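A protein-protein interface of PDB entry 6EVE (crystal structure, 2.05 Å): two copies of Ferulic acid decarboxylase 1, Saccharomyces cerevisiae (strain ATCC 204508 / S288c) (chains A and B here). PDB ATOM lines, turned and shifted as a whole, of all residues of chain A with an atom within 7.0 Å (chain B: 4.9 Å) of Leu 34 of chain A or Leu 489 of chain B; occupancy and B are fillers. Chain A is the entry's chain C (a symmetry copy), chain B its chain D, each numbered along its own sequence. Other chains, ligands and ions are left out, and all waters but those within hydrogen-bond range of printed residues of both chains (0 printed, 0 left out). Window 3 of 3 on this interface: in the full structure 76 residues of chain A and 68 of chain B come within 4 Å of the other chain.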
ATOM      1  N   ILE A  30       7.098  -7.336  29.386  1.00  0.00           N
ATOM      2  CA  ILE A  30       7.410  -8.779  29.432  1.00  0.00           C
ATOM      3  C   ILE A  30       8.143  -9.064  30.721  1.00  0.00           C
ATOM      4  O   ILE A  30       9.027  -8.295  31.125  1.00  0.00           O
ATOM      5  CB  ILE A  30       8.318  -9.207  28.284  1.00  0.00           C
ATOM      6  CG1 ILE A  30       7.675  -8.902  26.954  1.00  0.00           C
ATOM      7  CG2 ILE A  30       8.654 -10.711  28.379  1.00  0.00           C
ATOM      8  CD1 ILE A  30       6.342  -9.613  26.719  1.00  0.00           C
ATOM      9  N   ASP A  31       7.758 -10.150  31.383  1.00  0.00           N
ATOM     10  CA  ASP A  31       8.361 -10.551  32.663  1.00  0.00           C
ATOM     11  C   ASP A  31       9.664 -11.318  32.383  1.00  0.00           C
ATOM     12  O   ASP A  31       9.643 -12.325  31.624  1.00  0.00           O
ATOM     13  CB  ASP A  31       7.381 -11.442  33.417  1.00  0.00           C
ATOM     14  CG  ASP A  31       7.654 -11.510  34.876  1.00  0.00           C
ATOM     15  OD1 ASP A  31       8.775 -11.241  35.342  1.00  0.00           O
ATOM     16  OD2 ASP A  31       6.704 -11.830  35.612  1.00  0.00           O
ATOM     17  N   PRO A  32      10.794 -10.872  32.971  1.00  0.00           N
ATOM     18  CA  PRO A  32      12.005 -11.719  32.860  1.00  0.00           C
ATOM     19  C   PRO A  32      11.846 -13.129  33.446  1.00  0.00           C
ATOM     20  O   PRO A  32      12.601 -14.026  33.091  1.00  0.00           O
ATOM     21  CB  PRO A  32      13.070 -10.926  33.657  1.00  0.00           C
ATOM     22  CG  PRO A  32      12.538  -9.535  33.732  1.00  0.00           C
ATOM     23  CD  PRO A  32      11.050  -9.648  33.747  1.00  0.00           C
ATOM     24  N   ASN A  33      10.914 -13.315  34.371  1.00  0.00           N
ATOM     25  CA  ASN A  33      10.563 -14.640  34.929  1.00  0.00           C
ATOM     26  C   ASN A  33       9.735 -15.501  33.939  1.00  0.00           C
ATOM     27  O   ASN A  33       8.575 -15.228  33.748  1.00  0.00           O
ATOM     28  CB  ASN A  33       9.831 -14.399  36.254  1.00  0.00           C
ATOM     29  CG  ASN A  33       9.506 -15.650  36.987  1.00  0.00           C
ATOM     30  OD1 ASN A  33      10.110 -16.684  36.800  1.00  0.00           O
ATOM     31  ND2 ASN A  33       8.535 -15.554  37.862  1.00  0.00           N
ATOM     32  N   LEU A  34      10.398 -16.469  33.286  1.00  0.00           N
ATOM     33  CA  LEU A  34       9.862 -17.446  32.246  1.00  0.00           C
ATOM     34  C   LEU A  34       9.461 -16.907  30.888  1.00  0.00           C
ATOM     35  O   LEU A  34       9.652 -17.587  29.879  1.00  0.00           O
ATOM     36  CB  LEU A  34       8.712 -18.347  32.798  1.00  0.00           C
ATOM     37  CG  LEU A  34       9.090 -19.268  33.991  1.00  0.00           C
ATOM     38  CD1 LEU A  34       7.871 -20.081  34.454  1.00  0.00           C
ATOM     39  CD2 LEU A  34      10.269 -20.198  33.641  1.00  0.00           C
ATOM     40  N   GLU A  35       8.850 -15.732  30.863  1.00  0.00           N
ATOM     41  CA  GLU A  35       8.186 -15.184  29.670  1.00  0.00           C
ATOM     42  C   GLU A  35       9.207 -14.927  28.538  1.00  0.00           C
ATOM     43  O   GLU A  35       9.017 -15.376  27.382  1.00  0.00           O
ATOM     44  CB  GLU A  35       7.437 -13.887  30.051  1.00  0.00           C
ATOM     45  CG  GLU A  35       5.962 -13.838  29.688  1.00  0.00           C
ATOM     46  CD  GLU A  35       5.132 -12.767  30.453  1.00  0.00           C
ATOM     47  OE1 GLU A  35       5.449 -11.554  30.331  1.00  0.00           O
ATOM     48  OE2 GLU A  35       4.098 -13.150  31.113  1.00  0.00           O
ATOM     49  N   VAL A  36      10.319 -14.241  28.886  1.00  0.00           N
ATOM     50  CA  VAL A  36      11.397 -14.018  27.942  1.00  0.00           C
ATOM     51  C   VAL A  36      11.800 -15.354  27.367  1.00  0.00           C
ATOM     52  O   VAL A  36      11.934 -15.489  26.129  1.00  0.00           O
ATOM     53  CB  VAL A  36      12.652 -13.388  28.621  1.00  0.00           C
ATOM     54  CG1 VAL A  36      13.916 -13.547  27.766  1.00  0.00           C
ATOM     55  CG2 VAL A  36      12.411 -11.935  28.940  1.00  0.00           C
ATOM     56  N   GLY A  37      12.084 -16.311  28.247  1.00  0.00           N
ATOM     57  CA  GLY A  37      12.565 -17.642  27.826  1.00  0.00           C
ATOM     58  C   GLY A  37      11.627 -18.428  26.895  1.00  0.00           C
ATOM     59  O   GLY A  37      12.068 -19.082  25.962  1.00  0.00           O
ATOM     60  N   ALA A  38      10.329 -18.371  27.151  1.00  0.00           N
ATOM     61  CA  ALA A  38       9.390 -19.115  26.323  1.00  0.00           C
ATOM     62  C   ALA A  38       9.258 -18.471  24.957  1.00  0.00           C
ATOM     63  O   ALA A  38       9.139 -19.157  23.942  1.00  0.00           O
ATOM     64  CB  ALA A  38       8.057 -19.202  27.031  1.00  0.00           C
ATOM     65  N   ILE A  39       9.325 -17.138  24.917  1.00  0.00           N
ATOM     66  CA  ILE A  39       9.223 -16.408  23.661  1.00  0.00           C
ATOM     67  C   ILE A  39      10.445 -16.793  22.776  1.00  0.00           C
ATOM     68  O   ILE A  39      10.301 -17.081  21.562  1.00  0.00           O
ATOM     69  CB  ILE A  39       9.062 -14.895  23.936  1.00  0.00           C
ATOM     70  CG1 ILE A  39       7.616 -14.601  24.362  1.00  0.00           C
ATOM     71  CG2 ILE A  39       9.355 -14.065  22.702  1.00  0.00           C
ATOM     72  CD1 ILE A  39       7.400 -13.233  25.001  1.00  0.00           C
ATOM     73  N   MET A  40      11.632 -16.832  23.407  1.00  0.00           N
ATOM     74  CA  MET A  40      12.871 -17.250  22.724  1.00  0.00           C
ATOM     75  C   MET A  40      12.781 -18.659  22.175  1.00  0.00           C
ATOM     76  O   MET A  40      13.084 -18.848  20.989  1.00  0.00           O
ATOM     77  CB  MET A  40      14.118 -17.091  23.621  1.00  0.00           C
ATOM     78  CG  MET A  40      14.437 -15.637  23.895  1.00  0.00           C
ATOM     79  SD  MET A  40      15.769 -15.434  25.109  1.00  0.00           S
ATOM     80  CE  MET A  40      17.030 -16.343  24.168  1.00  0.00           C
ATOM     81  N   PRO A 142      17.030 -12.575  33.568  1.00  0.00           N
ATOM     82  CA  PRO A 142      16.043 -13.621  33.204  1.00  0.00           C
ATOM     83  C   PRO A 142      16.110 -14.963  34.019  1.00  0.00           C
ATOM     84  O   PRO A 142      17.184 -15.367  34.382  1.00  0.00           O
ATOM     85  CB  PRO A 142      16.355 -13.880  31.736  1.00  0.00           C
ATOM     86  CG  PRO A 142      17.803 -13.541  31.577  1.00  0.00           C
ATOM     87  CD  PRO A 142      18.081 -12.439  32.543  1.00  0.00           C
ATOM     88  N   TYR A 143      14.945 -15.592  34.272  1.00  0.00           N
ATOM     89  CA  TYR A 143      14.796 -16.925  34.834  1.00  0.00           C
ATOM     90  C   TYR A 143      14.316 -17.741  33.643  1.00  0.00           C
ATOM     91  O   TYR A 143      13.141 -17.647  33.224  1.00  0.00           O
ATOM     92  CB  TYR A 143      13.804 -16.947  36.016  1.00  0.00           C
ATOM     93  CG  TYR A 143      13.700 -18.297  36.685  1.00  0.00           C
ATOM     94  CD1 TYR A 143      14.730 -18.775  37.481  1.00  0.00           C
ATOM     95  CD2 TYR A 143      12.580 -19.131  36.484  1.00  0.00           C
ATOM     96  CE1 TYR A 143      14.664 -20.027  38.064  1.00  0.00           C
ATOM     97  CE2 TYR A 143      12.493 -20.382  37.103  1.00  0.00           C
ATOM     98  CZ  TYR A 143      13.553 -20.846  37.843  1.00  0.00           C
ATOM     99  OH  TYR A 143      13.500 -22.078  38.444  1.00  0.00           O
ATOM    100  N   LEU A 144      15.238 -18.502  33.053  1.00  0.00           N
ATOM    101  CA  LEU A 144      15.090 -18.904  31.669  1.00  0.00           C
ATOM    102  C   LEU A 144      14.317 -20.248  31.461  1.00  0.00           C
ATOM    103  O   LEU A 144      13.513 -20.356  30.523  1.00  0.00           O
ATOM    104  CB  LEU A 144      16.467 -18.914  30.997  1.00  0.00           C
ATOM    105  CG  LEU A 144      17.115 -17.587  30.604  1.00  0.00           C
ATOM    106  CD1 LEU A 144      18.579 -17.786  30.159  1.00  0.00           C
ATOM    107  CD2 LEU A 144      16.297 -16.924  29.510  1.00  0.00           C
ATOM    108  N   HIS A 145      14.541 -21.239  32.317  1.00  0.00           N
ATOM    109  CA  HIS A 145      13.891 -22.540  32.212  1.00  0.00           C
ATOM    110  C   HIS A 145      13.164 -22.858  33.545  1.00  0.00           C
ATOM    111  O   HIS A 145      13.649 -22.465  34.655  1.00  0.00           O
ATOM    112  CB  HIS A 145      14.858 -23.702  31.964  1.00  0.00           C
ATOM    113  CG  HIS A 145      15.946 -23.447  30.974  1.00  0.00           C
ATOM    114  ND1 HIS A 145      15.913 -23.953  29.685  1.00  0.00           N
ATOM    115  CD2 HIS A 145      17.159 -22.844  31.111  1.00  0.00           C
ATOM    116  CE1 HIS A 145      17.038 -23.624  29.066  1.00  0.00           C
ATOM    117  NE2 HIS A 145      17.799 -22.940  29.906  1.00  0.00           N
ATOM    118  N   VAL A 146      12.012 -23.553  33.435  1.00  0.00           N
ATOM    119  CA  VAL A 146      11.368 -24.126  34.620  1.00  0.00           C
ATOM    120  C   VAL A 146      12.400 -25.041  35.335  1.00  0.00           C
ATOM    121  O   VAL A 146      13.138 -25.799  34.668  1.00  0.00           O
ATOM    122  CB  VAL A 146      10.075 -24.894  34.272  1.00  0.00           C
ATOM    123  CG1 VAL A 146       9.617 -25.770  35.438  1.00  0.00           C
ATOM    124  CG2 VAL A 146       8.979 -23.901  33.903  1.00  0.00           C
ATOM    125  N   SER A 147      12.504 -24.888  36.667  1.00  0.00           N
ATOM    126  CA  SER A 147      13.416 -25.657  37.505  1.00  0.00           C
ATOM    127  C   SER A 147      14.874 -25.270  37.487  1.00  0.00           C
ATOM    128  O   SER A 147      15.672 -25.965  38.067  1.00  0.00           O
ATOM    129  CB  SER A 147      13.339 -27.168  37.182  1.00  0.00           C
ATOM    130  OG  SER A 147      12.280 -27.687  37.916  1.00  0.00           O
ATOM    131  N   ASN A 318      19.199 -19.048  25.255  1.00  0.00           N
ATOM    132  CA  ASN A 318      18.399 -19.965  26.077  1.00  0.00           C
ATOM    133  C   ASN A 318      18.492 -21.378  25.538  1.00  0.00           C
ATOM    134  O   ASN A 318      17.731 -21.766  24.638  1.00  0.00           O
ATOM    135  CB  ASN A 318      16.963 -19.489  26.122  1.00  0.00           C
ATOM    136  CG  ASN A 318      16.124 -20.256  27.112  1.00  0.00           C
ATOM    137  OD1 ASN A 318      16.646 -20.885  28.044  1.00  0.00           O
ATOM    138  ND2 ASN A 318      14.782 -20.194  26.925  1.00  0.00           N
ATOM    139  N   TYR B 485       7.263 -25.302  29.309  1.00  0.00           N
ATOM    140  CA  TYR B 485       6.674 -24.138  30.029  1.00  0.00           C
ATOM    141  C   TYR B 485       5.235 -24.444  30.436  1.00  0.00           C
ATOM    142  O   TYR B 485       4.652 -25.318  29.834  1.00  0.00           O
ATOM    143  CB  TYR B 485       6.761 -22.889  29.136  1.00  0.00           C
ATOM    144  CG  TYR B 485       8.182 -22.481  28.977  1.00  0.00           C
ATOM    145  CD1 TYR B 485       8.821 -21.610  29.916  1.00  0.00           C
ATOM    146  CD2 TYR B 485       8.934 -22.964  27.910  1.00  0.00           C
ATOM    147  CE1 TYR B 485      10.191 -21.264  29.758  1.00  0.00           C
ATOM    148  CE2 TYR B 485      10.275 -22.659  27.764  1.00  0.00           C
ATOM    149  CZ  TYR B 485      10.908 -21.815  28.682  1.00  0.00           C
ATOM    150  OH  TYR B 485      12.255 -21.574  28.497  1.00  0.00           O
ATOM    151  N   PRO B 486       4.665 -23.770  31.454  1.00  0.00           N
ATOM    152  CA  PRO B 486       3.260 -24.136  31.764  1.00  0.00           C
ATOM    153  C   PRO B 486       2.269 -23.811  30.637  1.00  0.00           C
ATOM    154  O   PRO B 486       2.425 -22.802  29.939  1.00  0.00           O
ATOM    155  CB  PRO B 486       2.926 -23.281  32.999  1.00  0.00           C
ATOM    156  CG  PRO B 486       4.254 -22.899  33.587  1.00  0.00           C
ATOM    157  CD  PRO B 486       5.218 -22.829  32.438  1.00  0.00           C
ATOM    158  N   LYS B 487       1.209 -24.609  30.526  1.00  0.00           N
ATOM    159  CA  LYS B 487       0.220 -24.421  29.468  1.00  0.00           C
ATOM    160  C   LYS B 487      -0.343 -23.021  29.413  1.00  0.00           C
ATOM    161  O   LYS B 487      -0.536 -22.485  28.317  1.00  0.00           O
ATOM    162  CB  LYS B 487      -0.934 -25.447  29.585  1.00  0.00           C
ATOM    163  CG  LYS B 487      -1.517 -25.761  28.222  1.00  0.00           C
ATOM    164  CD  LYS B 487      -2.897 -26.392  28.328  1.00  0.00           C
ATOM    165  CE  LYS B 487      -3.500 -26.687  26.949  1.00  0.00           C
ATOM    166  NZ  LYS B 487      -3.005 -25.785  25.857  1.00  0.00           N
ATOM    167  N   GLY B 488      -0.620 -22.427  30.574  1.00  0.00           N
ATOM    168  CA  GLY B 488      -1.127 -21.047  30.681  1.00  0.00           C
ATOM    169  C   GLY B 488      -0.253 -20.005  30.004  1.00  0.00           C
ATOM    170  O   GLY B 488      -0.746 -19.059  29.345  1.00  0.00           O
ATOM    171  N   LEU B 489       1.056 -20.205  30.147  1.00  0.00           N
ATOM    172  CA  LEU B 489       2.069 -19.294  29.601  1.00  0.00           C
ATOM    173  C   LEU B 489       2.232 -19.576  28.112  1.00  0.00           C
ATOM    174  O   LEU B 489       2.351 -18.665  27.291  1.00  0.00           O
ATOM    175  CB  LEU B 489       3.425 -19.498  30.327  1.00  0.00           C
ATOM    176  CG  LEU B 489       4.595 -18.666  29.722  1.00  0.00           C
ATOM    177  CD1 LEU B 489       4.220 -17.184  29.661  1.00  0.00           C
ATOM    178  CD2 LEU B 489       5.910 -18.824  30.472  1.00  0.00           C
ATOM    179  N   VAL B 490       2.249 -20.848  27.755  1.00  0.00           N
ATOM    180  CA  VAL B 490       2.253 -21.239  26.317  1.00  0.00           C
ATOM    181  C   VAL B 490       1.040 -20.599  25.612  1.00  0.00           C
ATOM    182  O   VAL B 490       1.169 -20.045  24.558  1.00  0.00           O
ATOM    183  CB  VAL B 490       2.250 -22.786  26.157  1.00  0.00           C
ATOM    184  CG1 VAL B 490       1.983 -23.209  24.719  1.00  0.00           C
ATOM    185  CG2 VAL B 490       3.541 -23.375  26.666  1.00  0.00           C
ATOM    186  N   ASP B 491      -0.152 -20.706  26.195  1.00  0.00           N
ATOM    187  CA  ASP B 491      -1.362 -20.095  25.596  1.00  0.00           C
ATOM    188  C   ASP B 491      -1.253 -18.559  25.553  1.00  0.00           C
ATOM    189  O   ASP B 491      -1.596 -17.968  24.534  1.00  0.00           O
ATOM    190  CB  ASP B 491      -2.649 -20.531  26.328  1.00  0.00           C
ATOM    191  CG  ASP B 491      -3.095 -21.988  25.973  1.00  0.00           C
ATOM    192  OD1 ASP B 491      -2.531 -22.585  25.017  1.00  0.00           O
ATOM    193  OD2 ASP B 491      -3.981 -22.558  26.681  1.00  0.00           O
ATOM    194  N   LYS B 492      -0.783 -17.923  26.642  1.00  0.00           N
ATOM    195  CA  LYS B 492      -0.633 -16.497  26.636  1.00  0.00           C
ATOM    196  C   LYS B 492       0.321 -16.042  25.487  1.00  0.00           C
ATOM    197  O   LYS B 492       0.015 -15.087  24.754  1.00  0.00           O
ATOM    198  CB  LYS B 492      -0.150 -16.015  28.017  1.00  0.00           C
ATOM    199  CG  LYS B 492      -0.075 -14.522  28.110  1.00  0.00           C
ATOM    200  CD  LYS B 492       0.688 -14.075  29.336  1.00  0.00           C
ATOM    201  CE  LYS B 492       0.851 -12.573  29.257  1.00  0.00           C
ATOM    202  NZ  LYS B 492       1.305 -12.015  30.540  1.00  0.00           N
ATOM    203  N   VAL B 493       1.458 -16.729  25.317  1.00  0.00           N
ATOM    204  CA  VAL B 493       2.392 -16.352  24.279  1.00  0.00           C
ATOM    205  C   VAL B 493       1.771 -16.491  22.886  1.00  0.00           C
ATOM    206  O   VAL B 493       1.968 -15.620  22.045  1.00  0.00           O
ATOM    207  CB  VAL B 493       3.724 -17.130  24.368  1.00  0.00           C
ATOM    208  CG1 VAL B 493       4.553 -16.893  23.128  1.00  0.00           C
ATOM    209  CG2 VAL B 493       4.521 -16.680  25.599  1.00  0.00           C
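N of Asp 31 of chain A sits at hydrogen-bond distance from OE1 of Glu 35 of chain A (2.9 Å).
The backbone NH of Leu 34 of chain A lies within hydrogen-bond range of the backbone carbonyl oxygen of Tyr 143 of chain A, at 3.0 Å.
The backbone carbonyl oxygen (O) of Gly 37 of chain A sits at hydrogen-bond distance from the side-chain amide nitrogen (ND2) of Asn 318 of chain A, 3.1 Å away.
A ring nitrogen (NE2) of His 145 of chain A lies close to the side-chain amide oxygen (OD1) of Asn 318 of chain A (3.0 Å).
The side-chain hydroxyl (OH) of Tyr 485 of chain B sits at hydrogen-bond distance from the backbone carbonyl oxygen (O) of Leu 144 of chain A (2.7 Å).
The side-chain hydroxyl of Tyr 485 of chain B sits at hydrogen-bond distance from the side-chain amide nitrogen of Asn 318 of chain A (3.3 Å).
The side-chain amino group of Lys 492 of chain B lies within salt-bridge range of the side-chain carboxylate of Glu 35 of chain A (3.1 Å).
Among the printed residues, pairs that only touch across the chains: Leu 34 of chain A with Tyr 485 of chain B, Leu 34 of chain A with Leu 489 of chain B, Glu 35 of chain A with Leu 489 of chain B, Gly 37 of chain A with Tyr 485 of chain B, Ala 38 of chain A with Tyr 485 of chain B and Ile 39 of chain A with Val 493 of chain B.
Asp 31 of chain A touches none of the printed residues of chain B.
Leu 34 of chain A touches just these residues of chain B: Tyr 485 (3.7 Å) and Leu 489 (3.7 Å).
Val 36 of chain A touches none of the printed residues of chain B.
Printed residues of chain B within 4 Å of Ile 39 of chain A: Val 493.
Of the printed residues of chain A, Tyr 485 of chain B touches Leu 34, Gly 37, Ala 38, Leu 144 and Asn 318.
No residue of chain A comes within 4 Å of Gly 488 of chain B.
Leu 489 of chain B touches just these residues of chain A: Leu 34 and Glu 35.
Of the printed residues of chain A, Lys 492 of chain B touches Glu 35.
The nearest residue of chain B that does not touch Leu 34 of chain A is Pro 486 of chain B (4.3 Å).
The nearest residue of chain A that does not touch Leu 489 of chain B is Ala 38 of chain A (4.1 Å).
The nearest printed residue of chain A that does not touch Tyr 485 of chain B is His 145 of chain A (4.2 Å).
No position is printed for both chains.
Of the 9 pairs that touch across the chains among the printed residues, none has its exchanged pair printed and touching as well.
Of the 9 printed residues of chain B, 4 touch a printed residue of chain A.
Printed residues of chain B that touch a printed residue of chain A: Tyr 485, Leu 489, Lys 492 and Val 493.
Hydrophobic or aromatic side chains of chain B that line the printed part of chain A: Tyr 485, Leu 489 and Val 493.
Of the 18 printed residues of chain A, 7 touch a printed residue of chain B.
Hydrophobic or aromatic side chains of chain A within 4 Å of the printed part of chain B: Leu 34, Ala 38 and Ile 39.
Among the printed residues, 9 pairs touch across the chains.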
